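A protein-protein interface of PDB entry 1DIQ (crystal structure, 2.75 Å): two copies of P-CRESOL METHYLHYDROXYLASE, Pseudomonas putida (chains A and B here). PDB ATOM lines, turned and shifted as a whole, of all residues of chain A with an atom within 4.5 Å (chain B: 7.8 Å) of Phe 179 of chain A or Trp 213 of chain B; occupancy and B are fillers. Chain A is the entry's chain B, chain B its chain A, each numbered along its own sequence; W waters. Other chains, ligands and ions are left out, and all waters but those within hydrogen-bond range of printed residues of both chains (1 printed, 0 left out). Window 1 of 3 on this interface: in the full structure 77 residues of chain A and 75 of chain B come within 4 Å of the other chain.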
ATOM      1  N   THR A 165      20.227  12.219   1.551  1.00  0.00           N
ATOM      2  CA  THR A 165      19.809  12.807   0.276  1.00  0.00           C
ATOM      3  C   THR A 165      20.769  13.905  -0.195  1.00  0.00           C
ATOM      4  O   THR A 165      20.883  14.132  -1.392  1.00  0.00           O
ATOM      5  CB  THR A 165      18.380  13.344   0.370  1.00  0.00           C
ATOM      6  OG1 THR A 165      17.565  12.342   0.975  1.00  0.00           O
ATOM      7  CG2 THR A 165      17.801  13.694  -1.004  1.00  0.00           C
ATOM      8  N   ARG A 168      23.068  12.063  -1.917  1.00  0.00           N
ATOM      9  CA  ARG A 168      22.341  11.245  -2.909  1.00  0.00           C
ATOM     10  C   ARG A 168      22.378   9.719  -2.691  1.00  0.00           C
ATOM     11  O   ARG A 168      22.648   8.941  -3.614  1.00  0.00           O
ATOM     12  CB  ARG A 168      22.792  11.572  -4.322  1.00  0.00           C
ATOM     13  CG  ARG A 168      22.252  12.823  -4.855  1.00  0.00           C
ATOM     14  CD  ARG A 168      22.804  12.943  -6.214  1.00  0.00           C
ATOM     15  NE  ARG A 168      23.369  14.257  -6.451  1.00  0.00           N
ATOM     16  CZ  ARG A 168      24.572  14.494  -6.959  1.00  0.00           C
ATOM     17  NH1 ARG A 168      25.405  13.519  -7.302  1.00  0.00           N
ATOM     18  NH2 ARG A 168      24.908  15.745  -7.181  1.00  0.00           N
ATOM     19  N   GLU A 177      15.559   5.461  -4.988  1.00  0.00           N
ATOM     20  CA  GLU A 177      16.488   6.497  -5.428  1.00  0.00           C
ATOM     21  C   GLU A 177      15.940   7.755  -4.727  1.00  0.00           C
ATOM     22  O   GLU A 177      15.022   8.410  -5.210  1.00  0.00           O
ATOM     23  CB  GLU A 177      16.488   6.611  -6.955  1.00  0.00           C
ATOM     24  CG  GLU A 177      17.577   7.503  -7.559  1.00  0.00           C
ATOM     25  CD  GLU A 177      19.003   7.042  -7.241  1.00  0.00           C
ATOM     26  OE1 GLU A 177      19.720   7.793  -6.545  1.00  0.00           O
ATOM     27  OE2 GLU A 177      19.417   5.949  -7.696  1.00  0.00           O
ATOM     28  N   HIS A 178      16.461   7.997  -3.526  1.00  0.00           N
ATOM     29  CA  HIS A 178      16.057   9.089  -2.661  1.00  0.00           C
ATOM     30  C   HIS A 178      15.986  10.508  -3.208  1.00  0.00           C
ATOM     31  O   HIS A 178      15.043  11.248  -2.870  1.00  0.00           O
ATOM     32  CB  HIS A 178      16.895   9.079  -1.389  1.00  0.00           C
ATOM     33  CG  HIS A 178      16.709   7.860  -0.550  1.00  0.00           C
ATOM     34  ND1 HIS A 178      17.681   7.402   0.306  1.00  0.00           N
ATOM     35  CD2 HIS A 178      15.661   7.010  -0.422  1.00  0.00           C
ATOM     36  CE1 HIS A 178      17.243   6.326   0.928  1.00  0.00           C
ATOM     37  NE2 HIS A 178      16.021   6.066   0.504  1.00  0.00           N
ATOM     38  N   PHE A 179      16.960  10.895  -4.037  1.00  0.00           N
ATOM     39  CA  PHE A 179      16.957  12.237  -4.605  1.00  0.00           C
ATOM     40  C   PHE A 179      15.875  12.436  -5.681  1.00  0.00           C
ATOM     41  O   PHE A 179      15.459  13.576  -5.945  1.00  0.00           O
ATOM     42  CB  PHE A 179      18.359  12.662  -5.088  1.00  0.00           C
ATOM     43  CG  PHE A 179      18.439  14.106  -5.517  1.00  0.00           C
ATOM     44  CD1 PHE A 179      18.680  14.428  -6.862  1.00  0.00           C
ATOM     45  CD2 PHE A 179      18.074  15.140  -4.635  1.00  0.00           C
ATOM     46  CE1 PHE A 179      18.534  15.762  -7.344  1.00  0.00           C
ATOM     47  CE2 PHE A 179      17.920  16.481  -5.104  1.00  0.00           C
ATOM     48  CZ  PHE A 179      18.145  16.786  -6.457  1.00  0.00           C
ATOM     49  N   MET A 180      15.377  11.326  -6.236  1.00  0.00           N
ATOM     50  CA  MET A 180      14.323  11.340  -7.255  1.00  0.00           C
ATOM     51  C   MET A 180      12.999  11.711  -6.572  1.00  0.00           C
ATOM     52  O   MET A 180      12.179  12.420  -7.151  1.00  0.00           O
ATOM     53  CB  MET A 180      14.233   9.960  -7.912  1.00  0.00           C
ATOM     54  CG  MET A 180      13.319   9.828  -9.120  1.00  0.00           C
ATOM     55  SD  MET A 180      14.101  10.265 -10.667  1.00  0.00           S
ATOM     56  CE  MET A 180      15.176   8.831 -10.846  1.00  0.00           C
ATOM     57  N   MET A 181      12.874  11.323  -5.301  1.00  0.00           N
ATOM     58  CA  MET A 181      11.678  11.568  -4.493  1.00  0.00           C
ATOM     59  C   MET A 181      11.709  12.811  -3.624  1.00  0.00           C
ATOM     60  O   MET A 181      10.748  13.102  -2.917  1.00  0.00           O
ATOM     61  CB  MET A 181      11.349  10.341  -3.632  1.00  0.00           C
ATOM     62  CG  MET A 181      11.174   9.076  -4.422  1.00  0.00           C
ATOM     63  SD  MET A 181      10.156   9.221  -5.916  1.00  0.00           S
ATOM     64  CE  MET A 181      10.835   7.893  -6.837  1.00  0.00           C
ATOM     65  N   GLN A 182      12.827  13.528  -3.653  1.00  0.00           N
ATOM     66  CA  GLN A 182      12.981  14.764  -2.901  1.00  0.00           C
ATOM     67  C   GLN A 182      12.088  15.828  -3.564  1.00  0.00           C
ATOM     68  O   GLN A 182      11.904  15.824  -4.780  1.00  0.00           O
ATOM     69  CB  GLN A 182      14.465  15.171  -2.902  1.00  0.00           C
ATOM     70  CG  GLN A 182      14.848  16.454  -2.145  1.00  0.00           C
ATOM     71  CD  GLN A 182      14.728  17.706  -2.988  1.00  0.00           C
ATOM     72  OE1 GLN A 182      14.845  17.660  -4.207  1.00  0.00           O
ATOM     73  NE2 GLN A 182      14.437  18.819  -2.346  1.00  0.00           N
ATOM     74  N   LYS A 212       7.815  19.531  -7.821  1.00  0.00           N
ATOM     75  CA  LYS A 212       9.266  19.624  -7.765  1.00  0.00           C
ATOM     76  C   LYS A 212       9.976  20.854  -8.306  1.00  0.00           C
ATOM     77  O   LYS A 212      10.691  21.550  -7.569  1.00  0.00           O
ATOM     78  CB  LYS A 212       9.897  18.382  -8.427  1.00  0.00           C
ATOM     79  CG  LYS A 212      10.121  17.187  -7.519  1.00  0.00           C
ATOM     80  CD  LYS A 212      10.685  15.983  -8.272  1.00  0.00           C
ATOM     81  CE  LYS A 212      12.196  15.988  -8.349  1.00  0.00           C
ATOM     82  NZ  LYS A 212      12.890  15.467  -7.129  1.00  0.00           N
ATOM     83  N   ASP A 220      17.561  22.322  -6.879  1.00  0.00           N
ATOM     84  CA  ASP A 220      17.742  21.312  -5.818  1.00  0.00           C
ATOM     85  C   ASP A 220      18.993  20.467  -6.026  1.00  0.00           C
ATOM     86  O   ASP A 220      19.796  20.281  -5.097  1.00  0.00           O
ATOM     87  CB  ASP A 220      16.540  20.375  -5.734  1.00  0.00           C
ATOM     88  CG  ASP A 220      15.250  21.099  -5.436  1.00  0.00           C
ATOM     89  OD1 ASP A 220      14.747  21.032  -4.298  1.00  0.00           O
ATOM     90  OD2 ASP A 220      14.728  21.761  -6.348  1.00  0.00           O
ATOM     91  N   GLY A 221      19.177  20.033  -7.275  1.00  0.00           N
ATOM     92  CA  GLY A 221      20.315  19.221  -7.660  1.00  0.00           C
ATOM     93  C   GLY A 221      21.662  19.871  -7.476  1.00  0.00           C
ATOM     94  O   GLY A 221      22.629  19.194  -7.133  1.00  0.00           O
ATOM     95  N   THR A 224      23.027  19.353  -3.886  1.00  0.00           N
ATOM     96  CA  THR A 224      23.389  17.993  -3.477  1.00  0.00           C
ATOM     97  C   THR A 224      24.776  17.677  -3.969  1.00  0.00           C
ATOM     98  O   THR A 224      25.116  17.992  -5.114  1.00  0.00           O
ATOM     99  CB  THR A 224      22.380  16.926  -3.941  1.00  0.00           C
ATOM    100  OG1 THR A 224      22.407  16.805  -5.374  1.00  0.00           O
ATOM    101  CG2 THR A 224      20.975  17.302  -3.456  1.00  0.00           C
ATOM    102  N   PHE B 179      10.791  15.999 -17.837  1.00  0.00           N
ATOM    103  CA  PHE B 179      12.078  16.323 -17.232  1.00  0.00           C
ATOM    104  C   PHE B 179      12.514  15.302 -16.170  1.00  0.00           C
ATOM    105  O   PHE B 179      13.702  15.196 -15.849  1.00  0.00           O
ATOM    106  CB  PHE B 179      12.122  17.778 -16.724  1.00  0.00           C
ATOM    107  CG  PHE B 179      13.475  18.207 -16.222  1.00  0.00           C
ATOM    108  CD1 PHE B 179      13.669  18.468 -14.854  1.00  0.00           C
ATOM    109  CD2 PHE B 179      14.602  18.164 -17.071  1.00  0.00           C
ATOM    110  CE1 PHE B 179      14.974  18.660 -14.316  1.00  0.00           C
ATOM    111  CE2 PHE B 179      15.917  18.351 -16.557  1.00  0.00           C
ATOM    112  CZ  PHE B 179      16.101  18.594 -15.179  1.00  0.00           C
ATOM    113  N   MET B 180      11.559  14.505 -15.694  1.00  0.00           N
ATOM    114  CA  MET B 180      11.810  13.456 -14.697  1.00  0.00           C
ATOM    115  C   MET B 180      12.532  12.300 -15.413  1.00  0.00           C
ATOM    116  O   MET B 180      13.428  11.654 -14.852  1.00  0.00           O
ATOM    117  CB  MET B 180      10.474  12.978 -14.107  1.00  0.00           C
ATOM    118  CG  MET B 180      10.540  12.033 -12.922  1.00  0.00           C
ATOM    119  SD  MET B 180      10.702  12.875 -11.369  1.00  0.00           S
ATOM    120  CE  MET B 180       9.031  13.552 -11.195  1.00  0.00           C
ATOM    121  N   GLN B 182      14.430  12.730 -18.236  1.00  0.00           N
ATOM    122  CA  GLN B 182      15.600  13.237 -18.935  1.00  0.00           C
ATOM    123  C   GLN B 182      16.836  12.630 -18.252  1.00  0.00           C
ATOM    124  O   GLN B 182      16.823  12.386 -17.044  1.00  0.00           O
ATOM    125  CB  GLN B 182      15.593  14.773 -18.885  1.00  0.00           C
ATOM    126  CG  GLN B 182      16.775  15.507 -19.567  1.00  0.00           C
ATOM    127  CD  GLN B 182      17.987  15.663 -18.664  1.00  0.00           C
ATOM    128  OE1 GLN B 182      17.868  15.702 -17.438  1.00  0.00           O
ATOM    129  NE2 GLN B 182      19.157  15.699 -19.261  1.00  0.00           N
ATOM    130  N   CYS B 183      17.864  12.328 -19.045  1.00  0.00           N
ATOM    131  CA  CYS B 183      19.099  11.757 -18.531  1.00  0.00           C
ATOM    132  C   CYS B 183      20.311  12.136 -19.403  1.00  0.00           C
ATOM    133  O   CYS B 183      20.553  11.568 -20.482  1.00  0.00           O
ATOM    134  CB  CYS B 183      18.991  10.240 -18.387  1.00  0.00           C
ATOM    135  SG  CYS B 183      20.350   9.600 -17.428  1.00  0.00           S
ATOM    136  N   GLY B 184      21.068  13.114 -18.908  1.00  0.00           N
ATOM    137  CA  GLY B 184      22.240  13.592 -19.607  1.00  0.00           C
ATOM    138  C   GLY B 184      21.982  14.622 -20.700  1.00  0.00           C
ATOM    139  O   GLY B 184      21.057  14.488 -21.510  1.00  0.00           O
ATOM    140  N   TYR B 195      30.010  21.513 -21.978  1.00  0.00           N
ATOM    141  CA  TYR B 195      29.763  20.812 -20.723  1.00  0.00           C
ATOM    142  C   TYR B 195      28.761  19.671 -20.906  1.00  0.00           C
ATOM    143  O   TYR B 195      27.754  19.824 -21.606  1.00  0.00           O
ATOM    144  CB  TYR B 195      29.234  21.801 -19.682  1.00  0.00           C
ATOM    145  CG  TYR B 195      28.806  21.187 -18.351  1.00  0.00           C
ATOM    146  CD1 TYR B 195      29.740  20.558 -17.503  1.00  0.00           C
ATOM    147  CD2 TYR B 195      27.462  21.257 -17.918  1.00  0.00           C
ATOM    148  CE1 TYR B 195      29.345  20.019 -16.258  1.00  0.00           C
ATOM    149  CE2 TYR B 195      27.066  20.718 -16.662  1.00  0.00           C
ATOM    150  CZ  TYR B 195      28.023  20.104 -15.849  1.00  0.00           C
ATOM    151  OH  TYR B 195      27.687  19.583 -14.633  1.00  0.00           O
ATOM    152  N   THR B 197      26.515  16.995 -18.621  1.00  0.00           N
ATOM    153  CA  THR B 197      26.006  16.629 -17.299  1.00  0.00           C
ATOM    154  C   THR B 197      26.102  15.122 -16.993  1.00  0.00           C
ATOM    155  O   THR B 197      26.348  14.297 -17.892  1.00  0.00           O
ATOM    156  CB  THR B 197      24.543  17.013 -17.149  1.00  0.00           C
ATOM    157  OG1 THR B 197      23.762  16.355 -18.162  1.00  0.00           O
ATOM    158  CG2 THR B 197      24.361  18.508 -17.257  1.00  0.00           C
ATOM    159  N   GLY B 198      25.920  14.796 -15.713  1.00  0.00           N
ATOM    160  CA  GLY B 198      25.960  13.424 -15.255  1.00  0.00           C
ATOM    161  C   GLY B 198      27.246  12.672 -15.505  1.00  0.00           C
ATOM    162  O   GLY B 198      28.300  13.070 -15.049  1.00  0.00           O
ATOM    163  N   MET B 199      27.152  11.600 -16.278  1.00  0.00           N
ATOM    164  CA  MET B 199      28.292  10.740 -16.571  1.00  0.00           C
ATOM    165  C   MET B 199      29.035  11.088 -17.871  1.00  0.00           C
ATOM    166  O   MET B 199      29.988  10.408 -18.259  1.00  0.00           O
ATOM    167  CB  MET B 199      27.824   9.269 -16.602  1.00  0.00           C
ATOM    168  CG  MET B 199      27.160   8.729 -15.321  1.00  0.00           C
ATOM    169  SD  MET B 199      28.151   8.815 -13.810  1.00  0.00           S
ATOM    170  CE  MET B 199      29.526   7.787 -14.147  1.00  0.00           C
ATOM    171  N   THR B 207      27.552   5.326 -19.779  1.00  0.00           N
ATOM    172  CA  THR B 207      26.491   5.548 -18.801  1.00  0.00           C
ATOM    173  C   THR B 207      25.810   6.919 -18.759  1.00  0.00           C
ATOM    174  O   THR B 207      25.047   7.197 -17.833  1.00  0.00           O
ATOM    175  CB  THR B 207      26.961   5.178 -17.374  1.00  0.00           C
ATOM    176  OG1 THR B 207      28.257   5.748 -17.130  1.00  0.00           O
ATOM    177  CG2 THR B 207      26.992   3.677 -17.197  1.00  0.00           C
ATOM    178  N   TRP B 208      26.004   7.723 -19.800  1.00  0.00           N
ATOM    179  CA  TRP B 208      25.440   9.076 -19.902  1.00  0.00           C
ATOM    180  C   TRP B 208      23.914   9.116 -19.851  1.00  0.00           C
ATOM    181  O   TRP B 208      23.312  10.000 -19.228  1.00  0.00           O
ATOM    182  CB  TRP B 208      25.946   9.726 -21.194  1.00  0.00           C
ATOM    183  CG  TRP B 208      25.845  11.229 -21.288  1.00  0.00           C
ATOM    184  CD1 TRP B 208      25.718  12.123 -20.261  1.00  0.00           C
ATOM    185  CD2 TRP B 208      25.898  12.007 -22.487  1.00  0.00           C
ATOM    186  NE1 TRP B 208      25.692  13.406 -20.742  1.00  0.00           N
ATOM    187  CE2 TRP B 208      25.804  13.369 -22.106  1.00  0.00           C
ATOM    188  CE3 TRP B 208      26.034  11.687 -23.852  1.00  0.00           C
ATOM    189  CZ2 TRP B 208      25.838  14.420 -23.041  1.00  0.00           C
ATOM    190  CZ3 TRP B 208      26.075  12.739 -24.794  1.00  0.00           C
ATOM    191  CH2 TRP B 208      25.976  14.090 -24.375  1.00  0.00           C
ATOM    192  N   ILE B 210      22.191   6.485 -18.715  1.00  0.00           N
ATOM    193  CA  ILE B 210      21.877   5.435 -17.772  1.00  0.00           C
ATOM    194  C   ILE B 210      21.638   5.921 -16.336  1.00  0.00           C
ATOM    195  O   ILE B 210      20.611   5.607 -15.740  1.00  0.00           O
ATOM    196  CB  ILE B 210      22.987   4.334 -17.873  1.00  0.00           C
ATOM    197  CG1 ILE B 210      22.931   3.595 -19.228  1.00  0.00           C
ATOM    198  CG2 ILE B 210      23.011   3.419 -16.696  1.00  0.00           C
ATOM    199  CD1 ILE B 210      21.634   2.808 -19.513  1.00  0.00           C
ATOM    200  N   PHE B 211      22.595   6.670 -15.794  1.00  0.00           N
ATOM    201  CA  PHE B 211      22.528   7.217 -14.433  1.00  0.00           C
ATOM    202  C   PHE B 211      22.455   8.772 -14.511  1.00  0.00           C
ATOM    203  O   PHE B 211      23.361   9.454 -15.024  1.00  0.00           O
ATOM    204  CB  PHE B 211      23.752   6.718 -13.646  1.00  0.00           C
ATOM    205  CG  PHE B 211      23.782   7.121 -12.190  1.00  0.00           C
ATOM    206  CD1 PHE B 211      22.816   6.634 -11.284  1.00  0.00           C
ATOM    207  CD2 PHE B 211      24.797   7.997 -11.714  1.00  0.00           C
ATOM    208  CE1 PHE B 211      22.849   7.014  -9.909  1.00  0.00           C
ATOM    209  CE2 PHE B 211      24.846   8.381 -10.350  1.00  0.00           C
ATOM    210  CZ  PHE B 211      23.864   7.885  -9.439  1.00  0.00           C
ATOM    211  N   LYS B 212      21.369   9.310 -13.962  1.00  0.00           N
ATOM    212  CA  LYS B 212      21.079  10.736 -13.985  1.00  0.00           C
ATOM    213  C   LYS B 212      22.052  11.718 -13.363  1.00  0.00           C
ATOM    214  O   LYS B 212      22.524  12.633 -14.030  1.00  0.00           O
ATOM    215  CB  LYS B 212      19.695  11.002 -13.370  1.00  0.00           C
ATOM    216  CG  LYS B 212      18.528  10.974 -14.327  1.00  0.00           C
ATOM    217  CD  LYS B 212      17.202  11.148 -13.605  1.00  0.00           C
ATOM    218  CE  LYS B 212      16.795  12.595 -13.475  1.00  0.00           C
ATOM    219  NZ  LYS B 212      16.122  13.158 -14.682  1.00  0.00           N
ATOM    220  N   TRP B 213      22.358  11.493 -12.092  1.00  0.00           N
ATOM    221  CA  TRP B 213      23.159  12.409 -11.290  1.00  0.00           C
ATOM    222  C   TRP B 213      24.629  12.651 -11.550  1.00  0.00           C
ATOM    223  O   TRP B 213      25.048  13.797 -11.649  1.00  0.00           O
ATOM    224  CB  TRP B 213      22.955  12.123  -9.792  1.00  0.00           C
ATOM    225  CG  TRP B 213      21.618  11.531  -9.363  1.00  0.00           C
ATOM    226  CD1 TRP B 213      21.443  10.386  -8.640  1.00  0.00           C
ATOM    227  CD2 TRP B 213      20.299  12.058  -9.597  1.00  0.00           C
ATOM    228  NE1 TRP B 213      20.115  10.162  -8.401  1.00  0.00           N
ATOM    229  CE2 TRP B 213      19.382  11.162  -8.978  1.00  0.00           C
ATOM    230  CE3 TRP B 213      19.794  13.198 -10.262  1.00  0.00           C
ATOM    231  CZ2 TRP B 213      17.990  11.362  -9.009  1.00  0.00           C
ATOM    232  CZ3 TRP B 213      18.407  13.399 -10.290  1.00  0.00           C
ATOM    233  CH2 TRP B 213      17.522  12.478  -9.666  1.00  0.00           C
ATOM    234  N   GLY B 214      25.401  11.575 -11.621  1.00  0.00           N
ATOM    235  CA  GLY B 214      26.827  11.673 -11.807  1.00  0.00           C
ATOM    236  C   GLY B 214      27.439  11.814 -10.421  1.00  0.00           C
ATOM    237  O   GLY B 214      27.065  11.090  -9.485  1.00  0.00           O
ATOM    238  N   TYR B 215      28.334  12.794 -10.288  1.00  0.00           N
ATOM    239  CA  TYR B 215      29.035  13.077  -9.038  1.00  0.00           C
ATOM    240  C   TYR B 215      29.179  14.585  -8.927  1.00  0.00           C
ATOM    241  O   TYR B 215      29.322  15.252  -9.934  1.00  0.00           O
ATOM    242  CB  TYR B 215      30.393  12.378  -9.065  1.00  0.00           C
ATOM    243  CG  TYR B 215      31.359  12.775  -8.007  1.00  0.00           C
ATOM    244  CD1 TYR B 215      32.333  13.774  -8.264  1.00  0.00           C
ATOM    245  CD2 TYR B 215      31.304  12.189  -6.721  1.00  0.00           C
ATOM    246  CE1 TYR B 215      33.231  14.186  -7.258  1.00  0.00           C
ATOM    247  CE2 TYR B 215      32.203  12.593  -5.709  1.00  0.00           C
ATOM    248  CZ  TYR B 215      33.159  13.592  -6.001  1.00  0.00           C
ATOM    249  OH  TYR B 215      34.047  13.976  -5.060  1.00  0.00           O
ATOM    250  N   GLY B 216      29.199  15.102  -7.696  1.00  0.00           N
ATOM    251  CA  GLY B 216      29.290  16.537  -7.474  1.00  0.00           C
ATOM    252  C   GLY B 216      27.924  17.152  -7.738  1.00  0.00           C
ATOM    253  O   GLY B 216      26.986  16.395  -7.867  1.00  0.00           O
ATOM    254  N   PRO B 217      27.760  18.482  -7.849  1.00  0.00           N
ATOM    255  CA  PRO B 217      26.413  19.009  -8.107  1.00  0.00           C
ATOM    256  C   PRO B 217      25.830  18.509  -9.427  1.00  0.00           C
ATOM    257  O   PRO B 217      26.573  18.283 -10.387  1.00  0.00           O
ATOM    258  CB  PRO B 217      26.628  20.525  -8.109  1.00  0.00           C
ATOM    259  CG  PRO B 217      28.062  20.686  -8.390  1.00  0.00           C
ATOM    260  CD  PRO B 217      28.721  19.575  -7.651  1.00  0.00           C
ATOM    261  N   THR B 218      24.536  18.194  -9.425  1.00  0.00           N
ATOM    262  CA  THR B 218      23.885  17.720 -10.642  1.00  0.00           C
ATOM    263  C   THR B 218      23.125  18.899 -11.234  1.00  0.00           C
ATOM    264  O   THR B 218      22.128  19.381 -10.675  1.00  0.00           O
ATOM    265  CB  THR B 218      23.053  16.407 -10.427  1.00  0.00           C
ATOM    266  OG1 THR B 218      22.347  16.080 -11.628  1.00  0.00           O
ATOM    267  CG2 THR B 218      22.096  16.501  -9.264  1.00  0.00           C
ATOM    268  N   LEU B 219      23.675  19.384 -12.347  1.00  0.00           N
ATOM    269  CA  LEU B 219      23.196  20.577 -13.043  1.00  0.00           C
ATOM    270  C   LEU B 219      22.164  20.585 -14.177  1.00  0.00           C
ATOM    271  O   LEU B 219      21.860  21.657 -14.691  1.00  0.00           O
ATOM    272  CB  LEU B 219      24.418  21.411 -13.473  1.00  0.00           C
ATOM    273  CG  LEU B 219      25.273  22.258 -12.511  1.00  0.00           C
ATOM    274  CD1 LEU B 219      24.794  22.255 -11.077  1.00  0.00           C
ATOM    275  CD2 LEU B 219      26.676  21.761 -12.585  1.00  0.00           C
ATOM    276  N   ASP B 220      21.606  19.446 -14.563  1.00  0.00           N
ATOM    277  CA  ASP B 220      20.598  19.408 -15.640  1.00  0.00           C
ATOM    278  C   ASP B 220      19.448  20.399 -15.435  1.00  0.00           C
ATOM    279  O   ASP B 220      19.092  21.140 -16.360  1.00  0.00           O
ATOM    280  CB  ASP B 220      19.995  18.013 -15.773  1.00  0.00           C
ATOM    281  CG  ASP B 220      21.023  16.974 -16.053  1.00  0.00           C
ATOM    282  OD1 ASP B 220      21.094  16.507 -17.216  1.00  0.00           O
ATOM    283  OD2 ASP B 220      21.782  16.641 -15.112  1.00  0.00           O
ATOM    284  N   TRP B 237      14.957   8.762 -21.246  1.00  0.00           N
ATOM    285  CA  TRP B 237      14.504   7.376 -21.159  1.00  0.00           C
ATOM    286  C   TRP B 237      13.191   7.167 -21.906  1.00  0.00           C
ATOM    287  O   TRP B 237      12.312   8.039 -21.897  1.00  0.00           O
ATOM    288  CB  TRP B 237      14.325   6.993 -19.703  1.00  0.00           C
ATOM    289  CG  TRP B 237      15.582   7.037 -18.863  1.00  0.00           C
ATOM    290  CD1 TRP B 237      16.862   6.778 -19.269  1.00  0.00           C
ATOM    291  CD2 TRP B 237      15.657   7.306 -17.452  1.00  0.00           C
ATOM    292  NE1 TRP B 237      17.734   6.854 -18.199  1.00  0.00           N
ATOM    293  CE2 TRP B 237      17.027   7.186 -17.074  1.00  0.00           C
ATOM    294  CE3 TRP B 237      14.703   7.642 -16.467  1.00  0.00           C
ATOM    295  CZ2 TRP B 237      17.470   7.394 -15.746  1.00  0.00           C
ATOM    296  CZ3 TRP B 237      15.141   7.852 -15.133  1.00  0.00           C
ATOM    297  CH2 TRP B 237      16.514   7.728 -14.792  1.00  0.00           C
HETATM  298  O   HOH W   1      25.514  10.241  -7.211  1.00  0.00           O
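5 positions are printed for both chains. Of the 13 pairs that touch across the chains among the printed residues, none has its exchanged pair printed and touching as well.
Among the printed residues, merely in contact across the chains: Arg 168 of chain A with Trp 213 of chain B (3.6 Å), Arg 168 of chain A with Gly 214 of chain B (3.7 Å), Arg 168 of chain A with Pro 217 of chain B (3.7 Å), Phe 179 of chain A with Trp 213 of chain B (3.6 Å), Met 180 of chain A with Trp 213 of chain B (3.8 Å), Gly 221 of chain A with Pro 217 of chain B (3.9 Å), Thr 224 of chain A with Gly 216 of chain B (3.7 Å), Thr 224 of chain A with Pro 217 of chain B (3.4 Å) and Thr 224 of chain A with Thr 218 of chain B (3.9 Å).
Water W1 lies within hydrogen-bond range of the backbone carbonyl oxygen of Gly 214 of chain B (2.9 Å) and the guanidinium group of Arg 168 of chain A (3.3 Å).
NE of Arg 168 of chain A is in hydrogen-bond range of OG1 of Thr 224 of chain A (2.9 Å). NZ of Lys 212 of chain A lies within hydrogen-bond range of O of Met 180 of chain A (3.1 Å). O of Phe 179 of chain A lies within hydrogen-bond range of NZ of Lys 212 of chain A. O of Gly 221 of chain A is in hydrogen-bond range of OG1 of Thr 224 of chain A (3.0 Å).
N of Thr 218 of chain B lies within hydrogen-bond range of O of Gly 221 of chain A (3.1 Å). The guanidinium group (NH2) of Arg 168 of chain A sits close to the backbone NH (N) of Thr 218 of chain B (3.3 Å). NE1 of Trp 213 of chain B sits at hydrogen-bond distance from OE1 of Glu 177 of chain A, 3.0 Å away. The backbone carbonyl oxygen (O) of Gly 216 of chain B lies close to the guanidinium group (NH1) of Arg 168 of chain A (3.3 Å).
Of chain B, only Trp 213 (3.6 Å) comes within 4 Å of Phe 179 of chain A. Of chain A, only Arg 168, Glu 177, Phe 179 and Met 180 come within 4 Å of Trp 213 of chain B. Printed residues of chain B within 4 Å of Thr 224 of chain A: Gly 216 (3.7 Å), Pro 217 (3.4 Å) and Thr 218 (3.9 Å). Printed residues of chain B within 4 Å of Arg 168 of chain A: Trp 213, Gly 214, Gly 216, Pro 217 and Thr 218. Met 181 of chain A touches none of the printed residues of chain B. The nearest residue of chain B that does not touch Phe 179 of chain A is Thr 218 of chain B (4.1 Å). The nearest printed residue of chain A that does not touch Trp 213 of chain B is Lys 212 of chain A (6.1 Å). The nearest printed residue of chain A that does not touch Gly 214 of chain B is Thr 224 of chain A (8.4 Å).
Of the 23 printed residues of chain B, 5 touch a printed residue of chain A. Hydrophobic or aromatic side chains of chain B within 4 Å of the printed part of chain A: Trp 213. Among the printed residues, 13 pairs touch across the chains. Among the printed residues, no Asp or Glu carboxylate lies within 4 Å of a Lys or Arg side-chain nitrogen of the other chain.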
